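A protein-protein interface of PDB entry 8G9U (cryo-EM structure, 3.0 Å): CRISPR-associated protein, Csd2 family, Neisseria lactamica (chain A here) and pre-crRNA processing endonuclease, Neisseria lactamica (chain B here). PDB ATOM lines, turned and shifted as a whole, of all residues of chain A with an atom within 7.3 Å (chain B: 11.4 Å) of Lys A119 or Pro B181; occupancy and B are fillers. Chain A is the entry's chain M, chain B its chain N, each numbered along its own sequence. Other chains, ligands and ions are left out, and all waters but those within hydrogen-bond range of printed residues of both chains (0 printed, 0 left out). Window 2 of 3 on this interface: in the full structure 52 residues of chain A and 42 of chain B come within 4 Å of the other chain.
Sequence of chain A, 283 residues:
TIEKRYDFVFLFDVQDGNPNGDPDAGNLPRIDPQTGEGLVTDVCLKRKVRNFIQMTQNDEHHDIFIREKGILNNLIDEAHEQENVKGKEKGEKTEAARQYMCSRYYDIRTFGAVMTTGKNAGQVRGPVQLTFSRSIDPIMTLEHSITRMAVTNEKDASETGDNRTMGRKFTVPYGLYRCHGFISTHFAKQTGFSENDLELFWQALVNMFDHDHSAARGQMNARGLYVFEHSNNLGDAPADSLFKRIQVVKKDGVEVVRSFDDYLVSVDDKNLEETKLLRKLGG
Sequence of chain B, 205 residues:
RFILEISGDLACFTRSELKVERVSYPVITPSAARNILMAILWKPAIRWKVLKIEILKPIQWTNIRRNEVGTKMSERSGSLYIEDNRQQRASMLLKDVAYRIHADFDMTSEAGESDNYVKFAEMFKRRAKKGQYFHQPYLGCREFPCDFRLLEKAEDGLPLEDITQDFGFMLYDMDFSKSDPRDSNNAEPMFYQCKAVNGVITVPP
The side-chain carboxylate of Asp B183 lies close to the side-chain amide oxygen of Asn A120 (2.9 Å).
The backbone carbonyl oxygen (O) of Ala A121 sits at hydrogen-bond distance from the side-chain amino group (NZ) of Lys B72 (3.2 Å).
O of Arg B182 sits close to O of Lys A119 (2.8 Å).
O of Lys A119 lies close to OD1 of Asp B183 (3.4 Å).
N of Met A115 lies within hydrogen-bond range of O of Gly A122 (2.7 Å).
The side-chain amide nitrogen (NE2) of Gln A123 sits close to the side-chain amide nitrogen (ND2) of Asn A120 (3.4 Å).
Among the printed residues, pairs that only touch across the chains: Met A115 with Met B73 (3.0 Å), Lys A119 with Pro B181 (3.8 Å), Ala A121 with Asp B183 (3.9 Å) and Asn A120 with Arg B182 (3.99 Å).
Of chain B, only Pro B181 (3.8 Å), Arg B182 (2.8 Å) and Asp B183 (3.4 Å) come within 4 Å of Lys A119.
Pro B181 touches one residue of chain A.
No residue of chain B comes within 4 Å of Thr A94.
Printed residues of chain B within 4 Å of Ala A121: Lys B72 and Asp B183.
Gly A122 touches none of the printed residues of chain B.
Printed residues of chain A within 4 Å of Met B73: Met A115 (3.0 Å).
Of the printed residues of chain A, Lys B72 touches Ala A121.
Asn B186 touches none of the printed residues of chain A.
The nearest printed residue of chain A that does not touch Arg B182 is Ala A121 (5.0 Å).
Printed residues of chain B that touch a printed residue of chain A: Lys B72, Met B73, Pro B181, Arg B182 and Asp B183.
Along chain B the printed residues that touch a printed residue of chain A span positions 72 to 183.
Of the 12 printed residues of chain A, 4 touch a printed residue of chain B.
Printed residues of chain A that touch a printed residue of chain B: Met A115, Lys A119, Asn A120 and Ala A121.
Among the printed residues, no Asp or Glu carboxylate lies within 4 Å of a Lys or Arg side-chain nitrogen of the other chain.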
ATOM      1  N   THR A  94      -4.150 -17.742  20.692  1.00  0.00           N
ATOM      2  CA  THR A  94      -4.900 -18.950  21.016  1.00  0.00           C
ATOM      3  C   THR A  94      -5.080 -19.826  19.783  1.00  0.00           C
ATOM      4  O   THR A  94      -4.906 -21.049  19.852  1.00  0.00           O
ATOM      5  CB  THR A  94      -6.254 -18.584  21.625  1.00  0.00           C
ATOM      6  OG1 THR A  94      -6.047 -17.904  22.869  1.00  0.00           O
ATOM      7  CG2 THR A  94      -7.089 -19.832  21.874  1.00  0.00           C
ATOM      8  N   GLU A  95      -5.414 -19.224  18.646  1.00  0.00           N
ATOM      9  CA  GLU A  95      -5.459 -19.948  17.377  1.00  0.00           C
ATOM     10  C   GLU A  95      -4.118 -19.858  16.659  1.00  0.00           C
ATOM     11  O   GLU A  95      -4.019 -19.542  15.474  1.00  0.00           O
ATOM     12  CB  GLU A  95      -6.591 -19.409  16.510  1.00  0.00           C
ATOM     13  CG  GLU A  95      -6.972 -20.281  15.316  1.00  0.00           C
ATOM     14  CD  GLU A  95      -7.604 -21.595  15.713  1.00  0.00           C
ATOM     15  OE1 GLU A  95      -8.084 -21.708  16.861  1.00  0.00           O
ATOM     16  OE2 GLU A  95      -7.634 -22.515  14.868  1.00  0.00           O
ATOM     17  N   ARG A  98      -3.266 -23.981  18.863  1.00  0.00           N
ATOM     18  CA  ARG A  98      -4.281 -24.943  18.453  1.00  0.00           C
ATOM     19  C   ARG A  98      -4.120 -25.324  16.990  1.00  0.00           C
ATOM     20  O   ARG A  98      -4.482 -26.437  16.600  1.00  0.00           O
ATOM     21  CB  ARG A  98      -5.675 -24.380  18.708  1.00  0.00           C
ATOM     22  CG  ARG A  98      -6.812 -25.303  18.309  1.00  0.00           C
ATOM     23  CD  ARG A  98      -7.388 -24.865  16.980  1.00  0.00           C
ATOM     24  NE  ARG A  98      -8.639 -25.526  16.640  1.00  0.00           N
ATOM     25  CZ  ARG A  98      -9.212 -25.446  15.447  1.00  0.00           C
ATOM     26  NH1 ARG A  98     -10.356 -26.070  15.214  1.00  0.00           N
ATOM     27  NH2 ARG A  98      -8.642 -24.735  14.486  1.00  0.00           N
ATOM     28  N   MET A 115      -8.481 -29.281  23.126  1.00  0.00           N
ATOM     29  CA  MET A 115      -7.352 -28.519  23.648  1.00  0.00           C
ATOM     30  C   MET A 115      -7.710 -27.688  24.869  1.00  0.00           C
ATOM     31  O   MET A 115      -8.658 -26.906  24.848  1.00  0.00           O
ATOM     32  CB  MET A 115      -6.796 -27.620  22.553  1.00  0.00           C
ATOM     33  CG  MET A 115      -6.375 -28.411  21.372  1.00  0.00           C
ATOM     34  SD  MET A 115      -4.694 -28.906  21.727  1.00  0.00           S
ATOM     35  CE  MET A 115      -4.698 -30.571  21.097  1.00  0.00           C
ATOM     36  N   THR A 117      -6.739 -25.147  26.251  1.00  0.00           N
ATOM     37  CA  THR A 117      -7.052 -23.804  25.803  1.00  0.00           C
ATOM     38  C   THR A 117      -7.615 -23.897  24.393  1.00  0.00           C
ATOM     39  O   THR A 117      -7.134 -24.682  23.572  1.00  0.00           O
ATOM     40  CB  THR A 117      -5.818 -22.897  25.847  1.00  0.00           C
ATOM     41  OG1 THR A 117      -6.201 -21.546  25.561  1.00  0.00           O
ATOM     42  CG2 THR A 117      -4.754 -23.346  24.852  1.00  0.00           C
ATOM     43  N   GLY A 118      -8.663 -23.135  24.130  1.00  0.00           N
ATOM     44  CA  GLY A 118      -9.291 -23.218  22.832  1.00  0.00           C
ATOM     45  C   GLY A 118     -10.320 -22.129  22.663  1.00  0.00           C
ATOM     46  O   GLY A 118     -10.414 -21.205  23.471  1.00  0.00           O
ATOM     47  N   LYS A 119     -11.086 -22.243  21.582  1.00  0.00           N
ATOM     48  CA  LYS A 119     -12.185 -21.316  21.352  1.00  0.00           C
ATOM     49  C   LYS A 119     -13.469 -21.849  21.970  1.00  0.00           C
ATOM     50  O   LYS A 119     -14.026 -21.239  22.886  1.00  0.00           O
ATOM     51  CB  LYS A 119     -12.368 -21.070  19.852  1.00  0.00           C
ATOM     52  CG  LYS A 119     -11.218 -20.333  19.206  1.00  0.00           C
ATOM     53  CD  LYS A 119     -11.017 -18.972  19.836  1.00  0.00           C
ATOM     54  CE  LYS A 119     -12.036 -17.975  19.331  1.00  0.00           C
ATOM     55  NZ  LYS A 119     -11.875 -16.638  19.961  1.00  0.00           N
ATOM     56  N   ASN A 120     -13.929 -23.006  21.503  1.00  0.00           N
ATOM     57  CA  ASN A 120     -15.159 -23.602  22.012  1.00  0.00           C
ATOM     58  C   ASN A 120     -14.877 -24.383  23.291  1.00  0.00           C
ATOM     59  O   ASN A 120     -15.075 -25.593  23.379  1.00  0.00           O
ATOM     60  CB  ASN A 120     -15.802 -24.484  20.957  1.00  0.00           C
ATOM     61  CG  ASN A 120     -16.305 -23.701  19.784  1.00  0.00           C
ATOM     62  OD1 ASN A 120     -17.190 -22.862  19.910  1.00  0.00           O
ATOM     63  ND2 ASN A 120     -15.726 -23.957  18.626  1.00  0.00           N
ATOM     64  N   ALA A 121     -14.381 -23.654  24.288  1.00  0.00           N
ATOM     65  CA  ALA A 121     -14.045 -24.220  25.590  1.00  0.00           C
ATOM     66  C   ALA A 121     -13.141 -25.432  25.452  1.00  0.00           C
ATOM     67  O   ALA A 121     -13.053 -26.265  26.355  1.00  0.00           O
ATOM     68  CB  ALA A 121     -15.301 -24.571  26.388  1.00  0.00           C
ATOM     69  N   GLY A 122     -12.474 -25.551  24.315  1.00  0.00           N
ATOM     70  CA  GLY A 122     -11.512 -26.605  24.146  1.00  0.00           C
ATOM     71  C   GLY A 122     -11.535 -27.311  22.814  1.00  0.00           C
ATOM     72  O   GLY A 122     -10.475 -27.678  22.304  1.00  0.00           O
ATOM     73  N   GLN A 123     -12.707 -27.490  22.216  1.00  0.00           N
ATOM     74  CA  GLN A 123     -12.812 -28.513  21.191  1.00  0.00           C
ATOM     75  C   GLN A 123     -12.038 -28.139  19.941  1.00  0.00           C
ATOM     76  O   GLN A 123     -11.953 -26.973  19.553  1.00  0.00           O
ATOM     77  CB  GLN A 123     -14.248 -28.777  20.778  1.00  0.00           C
ATOM     78  CG  GLN A 123     -14.920 -27.647  20.105  1.00  0.00           C
ATOM     79  CD  GLN A 123     -16.338 -27.975  19.778  1.00  0.00           C
ATOM     80  OE1 GLN A 123     -16.795 -29.087  20.021  1.00  0.00           O
ATOM     81  NE2 GLN A 123     -17.044 -27.021  19.196  1.00  0.00           N
ATOM     82  N   VAL A 124     -11.445 -29.156  19.337  1.00  0.00           N
ATOM     83  CA  VAL A 124     -11.228 -29.230  17.906  1.00  0.00           C
ATOM     84  C   VAL A 124     -11.955 -30.484  17.467  1.00  0.00           C
ATOM     85  O   VAL A 124     -11.638 -31.577  17.941  1.00  0.00           O
ATOM     86  CB  VAL A 124      -9.741 -29.300  17.549  1.00  0.00           C
ATOM     87  CG1 VAL A 124      -9.556 -29.052  16.081  1.00  0.00           C
ATOM     88  CG2 VAL A 124      -8.960 -28.299  18.368  1.00  0.00           C
ATOM     89  N   TRP B  42     -25.302 -24.202   9.605  1.00  0.00           N
ATOM     90  CA  TRP B  42     -25.242 -23.067  10.496  1.00  0.00           C
ATOM     91  C   TRP B  42     -24.441 -21.975   9.811  1.00  0.00           C
ATOM     92  O   TRP B  42     -23.829 -22.182   8.763  1.00  0.00           O
ATOM     93  CB  TRP B  42     -24.660 -23.449  11.856  1.00  0.00           C
ATOM     94  CG  TRP B  42     -24.765 -22.352  12.835  1.00  0.00           C
ATOM     95  CD1 TRP B  42     -25.873 -21.960  13.516  1.00  0.00           C
ATOM     96  CD2 TRP B  42     -23.723 -21.464  13.215  1.00  0.00           C
ATOM     97  NE1 TRP B  42     -25.580 -20.892  14.317  1.00  0.00           N
ATOM     98  CE2 TRP B  42     -24.263 -20.564  14.145  1.00  0.00           C
ATOM     99  CE3 TRP B  42     -22.382 -21.343  12.860  1.00  0.00           C
ATOM    100  CZ2 TRP B  42     -23.508 -19.562  14.724  1.00  0.00           C
ATOM    101  CZ3 TRP B  42     -21.639 -20.353  13.433  1.00  0.00           C
ATOM    102  CH2 TRP B  42     -22.198 -19.471  14.352  1.00  0.00           C
ATOM    103  N   PRO B  44     -23.143 -17.674  11.246  1.00  0.00           N
ATOM    104  CA  PRO B  44     -23.426 -16.681  12.283  1.00  0.00           C
ATOM    105  C   PRO B  44     -24.426 -15.650  11.794  1.00  0.00           C
ATOM    106  O   PRO B  44     -24.289 -14.457  12.057  1.00  0.00           O
ATOM    107  CB  PRO B  44     -22.054 -16.060  12.557  1.00  0.00           C
ATOM    108  CG  PRO B  44     -21.305 -16.257  11.295  1.00  0.00           C
ATOM    109  CD  PRO B  44     -21.765 -17.572  10.747  1.00  0.00           C
ATOM    110  N   LYS B  72      -8.121 -32.927  29.503  1.00  0.00           N
ATOM    111  CA  LYS B  72      -8.069 -32.236  28.230  1.00  0.00           C
ATOM    112  C   LYS B  72      -6.709 -32.444  27.592  1.00  0.00           C
ATOM    113  O   LYS B  72      -5.732 -32.827  28.236  1.00  0.00           O
ATOM    114  CB  LYS B  72      -8.274 -30.729  28.380  1.00  0.00           C
ATOM    115  CG  LYS B  72      -9.473 -30.239  29.142  1.00  0.00           C
ATOM    116  CD  LYS B  72     -10.530 -29.659  28.218  1.00  0.00           C
ATOM    117  CE  LYS B  72     -11.701 -29.123  29.013  1.00  0.00           C
ATOM    118  NZ  LYS B  72     -12.881 -28.850  28.161  1.00  0.00           N
ATOM    119  N   MET B  73      -6.655 -32.166  26.309  1.00  0.00           N
ATOM    120  CA  MET B  73      -5.400 -32.007  25.613  1.00  0.00           C
ATOM    121  C   MET B  73      -4.910 -30.577  25.709  1.00  0.00           C
ATOM    122  O   MET B  73      -5.693 -29.652  25.895  1.00  0.00           O
ATOM    123  CB  MET B  73      -5.574 -32.484  24.186  1.00  0.00           C
ATOM    124  CG  MET B  73      -6.341 -33.762  24.231  1.00  0.00           C
ATOM    125  SD  MET B  73      -6.211 -34.718  22.748  1.00  0.00           S
ATOM    126  CE  MET B  73      -7.678 -34.217  21.950  1.00  0.00           C
ATOM    127  N   SER B 109     -27.927 -11.034  15.393  1.00  0.00           N
ATOM    128  CA  SER B 109     -27.518  -9.648  15.222  1.00  0.00           C
ATOM    129  C   SER B 109     -26.551  -9.506  14.056  1.00  0.00           C
ATOM    130  O   SER B 109     -26.617  -8.529  13.302  1.00  0.00           O
ATOM    131  CB  SER B 109     -26.888  -9.129  16.511  1.00  0.00           C
ATOM    132  OG  SER B 109     -25.734  -9.877  16.844  1.00  0.00           O
ATOM    133  N   GLU B 110     -25.646 -10.463  13.895  1.00  0.00           N
ATOM    134  CA  GLU B 110     -24.671 -10.426  12.808  1.00  0.00           C
ATOM    135  C   GLU B 110     -25.174 -11.182  11.580  1.00  0.00           C
ATOM    136  O   GLU B 110     -24.485 -12.024  11.009  1.00  0.00           O
ATOM    137  CB  GLU B 110     -23.332 -10.972  13.295  1.00  0.00           C
ATOM    138  CG  GLU B 110     -23.390 -12.357  13.929  1.00  0.00           C
ATOM    139  CD  GLU B 110     -23.595 -12.325  15.429  1.00  0.00           C
ATOM    140  OE1 GLU B 110     -23.767 -11.221  15.987  1.00  0.00           O
ATOM    141  OE2 GLU B 110     -23.595 -13.409  16.049  1.00  0.00           O
ATOM    142  N   ASP B 175     -26.431 -21.454  27.516  1.00  0.00           N
ATOM    143  CA  ASP B 175     -26.662 -20.044  27.216  1.00  0.00           C
ATOM    144  C   ASP B 175     -25.357 -19.397  26.785  1.00  0.00           C
ATOM    145  O   ASP B 175     -24.535 -19.019  27.619  1.00  0.00           O
ATOM    146  CB  ASP B 175     -27.244 -19.333  28.430  1.00  0.00           C
ATOM    147  CG  ASP B 175     -27.377 -17.842  28.225  1.00  0.00           C
ATOM    148  OD1 ASP B 175     -27.530 -17.412  27.065  1.00  0.00           O
ATOM    149  OD2 ASP B 175     -27.338 -17.097  29.226  1.00  0.00           O
ATOM    150  N   PHE B 176     -25.165 -19.258  25.482  1.00  0.00           N
ATOM    151  CA  PHE B 176     -23.994 -18.565  24.948  1.00  0.00           C
ATOM    152  C   PHE B 176     -24.299 -17.106  24.658  1.00  0.00           C
ATOM    153  O   PHE B 176     -24.026 -16.597  23.575  1.00  0.00           O
ATOM    154  CB  PHE B 176     -23.503 -19.277  23.705  1.00  0.00           C
ATOM    155  CG  PHE B 176     -23.335 -20.739  23.899  1.00  0.00           C
ATOM    156  CD1 PHE B 176     -22.338 -21.222  24.706  1.00  0.00           C
ATOM    157  CD2 PHE B 176     -24.198 -21.628  23.310  1.00  0.00           C
ATOM    158  CE1 PHE B 176     -22.184 -22.558  24.890  1.00  0.00           C
ATOM    159  CE2 PHE B 176     -24.048 -22.971  23.504  1.00  0.00           C
ATOM    160  CZ  PHE B 176     -23.040 -23.433  24.291  1.00  0.00           C
ATOM    161  N   SER B 177     -24.863 -16.410  25.635  1.00  0.00           N
ATOM    162  CA  SER B 177     -25.127 -14.993  25.458  1.00  0.00           C
ATOM    163  C   SER B 177     -23.986 -14.145  25.985  1.00  0.00           C
ATOM    164  O   SER B 177     -23.525 -13.231  25.295  1.00  0.00           O
ATOM    165  CB  SER B 177     -26.432 -14.606  26.153  1.00  0.00           C
ATOM    166  OG  SER B 177     -26.331 -14.781  27.553  1.00  0.00           O
ATOM    167  N   LYS B 178     -23.516 -14.435  27.199  1.00  0.00           N
ATOM    168  CA  LYS B 178     -22.371 -13.728  27.751  1.00  0.00           C
ATOM    169  C   LYS B 178     -21.084 -14.057  27.020  1.00  0.00           C
ATOM    170  O   LYS B 178     -20.074 -13.378  27.235  1.00  0.00           O
ATOM    171  CB  LYS B 178     -22.211 -14.055  29.233  1.00  0.00           C
ATOM    172  CG  LYS B 178     -23.284 -13.465  30.115  1.00  0.00           C
ATOM    173  CD  LYS B 178     -23.103 -13.912  31.548  1.00  0.00           C
ATOM    174  CE  LYS B 178     -23.253 -15.417  31.664  1.00  0.00           C
ATOM    175  NZ  LYS B 178     -24.591 -15.874  31.202  1.00  0.00           N
ATOM    176  N   SER B 179     -21.095 -15.076  26.173  1.00  0.00           N
ATOM    177  CA  SER B 179     -19.890 -15.478  25.475  1.00  0.00           C
ATOM    178  C   SER B 179     -19.493 -14.467  24.410  1.00  0.00           C
ATOM    179  O   SER B 179     -20.335 -13.841  23.762  1.00  0.00           O
ATOM    180  CB  SER B 179     -20.089 -16.841  24.833  1.00  0.00           C
ATOM    181  OG  SER B 179     -20.037 -17.867  25.806  1.00  0.00           O
ATOM    182  N   ASP B 180     -18.188 -14.320  24.235  1.00  0.00           N
ATOM    183  CA  ASP B 180     -17.588 -13.610  23.119  1.00  0.00           C
ATOM    184  C   ASP B 180     -17.708 -14.529  21.910  1.00  0.00           C
ATOM    185  O   ASP B 180     -18.298 -15.609  22.038  1.00  0.00           O
ATOM    186  CB  ASP B 180     -16.134 -13.257  23.438  1.00  0.00           C
ATOM    187  CG  ASP B 180     -15.354 -14.438  23.971  1.00  0.00           C
ATOM    188  OD1 ASP B 180     -15.817 -15.584  23.805  1.00  0.00           O
ATOM    189  OD2 ASP B 180     -14.276 -14.222  24.560  1.00  0.00           O
ATOM    190  N   PRO B 181     -17.214 -14.153  20.732  1.00  0.00           N
ATOM    191  CA  PRO B 181     -17.171 -15.119  19.632  1.00  0.00           C
ATOM    192  C   PRO B 181     -16.570 -16.441  20.087  1.00  0.00           C
ATOM    193  O   PRO B 181     -15.560 -16.474  20.793  1.00  0.00           O
ATOM    194  CB  PRO B 181     -16.297 -14.423  18.591  1.00  0.00           C
ATOM    195  CG  PRO B 181     -16.549 -12.979  18.813  1.00  0.00           C
ATOM    196  CD  PRO B 181     -16.938 -12.784  20.255  1.00  0.00           C
ATOM    197  N   ARG B 182     -17.224 -17.533  19.693  1.00  0.00           N
ATOM    198  CA  ARG B 182     -16.845 -18.894  20.055  1.00  0.00           C
ATOM    199  C   ARG B 182     -17.016 -19.168  21.549  1.00  0.00           C
ATOM    200  O   ARG B 182     -16.042 -19.456  22.250  1.00  0.00           O
ATOM    201  CB  ARG B 182     -15.411 -19.194  19.619  1.00  0.00           C
ATOM    202  CG  ARG B 182     -15.163 -19.285  18.104  1.00  0.00           C
ATOM    203  CD  ARG B 182     -15.533 -18.017  17.336  1.00  0.00           C
ATOM    204  NE  ARG B 182     -15.102 -18.062  15.943  1.00  0.00           N
ATOM    205  CZ  ARG B 182     -14.934 -16.985  15.187  1.00  0.00           C
ATOM    206  NH1 ARG B 182     -14.533 -17.110  13.931  1.00  0.00           N
ATOM    207  NH2 ARG B 182     -15.165 -15.783  15.692  1.00  0.00           N
ATOM    208  N   ASP B 183     -18.249 -19.003  22.040  1.00  0.00           N
ATOM    209  CA  ASP B 183     -18.826 -19.544  23.278  1.00  0.00           C
ATOM    210  C   ASP B 183     -17.911 -19.702  24.492  1.00  0.00           C
ATOM    211  O   ASP B 183     -17.867 -20.778  25.097  1.00  0.00           O
ATOM    212  CB  ASP B 183     -19.502 -20.890  23.001  1.00  0.00           C
ATOM    213  CG  ASP B 183     -18.540 -21.985  22.630  1.00  0.00           C
ATOM    214  OD1 ASP B 183     -17.336 -21.733  22.576  1.00  0.00           O
ATOM    215  OD2 ASP B 183     -18.995 -23.120  22.394  1.00  0.00           O
ATOM    216  N   SER B 184     -17.239 -18.636  24.912  1.00  0.00           N
ATOM    217  CA  SER B 184     -16.332 -18.771  26.042  1.00  0.00           C
ATOM    218  C   SER B 184     -17.088 -18.966  27.347  1.00  0.00           C
ATOM    219  O   SER B 184     -17.020 -20.038  27.952  1.00  0.00           O
ATOM    220  CB  SER B 184     -15.432 -17.546  26.151  1.00  0.00           C
ATOM    221  OG  SER B 184     -14.837 -17.252  24.903  1.00  0.00           O
ATOM    222  N   ASN B 185     -17.839 -17.955  27.766  1.00  0.00           N
ATOM    223  CA  ASN B 185     -18.454 -17.914  29.090  1.00  0.00           C
ATOM    224  C   ASN B 185     -19.946 -18.134  28.922  1.00  0.00           C
ATOM    225  O   ASN B 185     -20.675 -17.219  28.535  1.00  0.00           O
ATOM    226  CB  ASN B 185     -18.176 -16.583  29.775  1.00  0.00           C
ATOM    227  CG  ASN B 185     -16.708 -16.363  30.037  1.00  0.00           C
ATOM    228  OD1 ASN B 185     -16.096 -15.458  29.472  1.00  0.00           O
ATOM    229  ND2 ASN B 185     -16.129 -17.199  30.889  1.00  0.00           N
ATOM    230  N   ASN B 186     -20.401 -19.333  29.225  1.00  0.00           N
ATOM    231  CA  ASN B 186     -21.789 -19.684  29.007  1.00  0.00           C
ATOM    232  C   ASN B 186     -22.500 -19.924  30.332  1.00  0.00           C
ATOM    233  O   ASN B 186     -21.946 -19.715  31.417  1.00  0.00           O
ATOM    234  CB  ASN B 186     -21.884 -20.916  28.121  1.00  0.00           C
ATOM    235  CG  ASN B 186     -21.671 -22.186  28.892  1.00  0.00           C
ATOM    236  OD1 ASN B 186     -20.789 -22.264  29.743  1.00  0.00           O
ATOM    237  ND2 ASN B 186     -22.503 -23.183  28.633  1.00  0.00           N
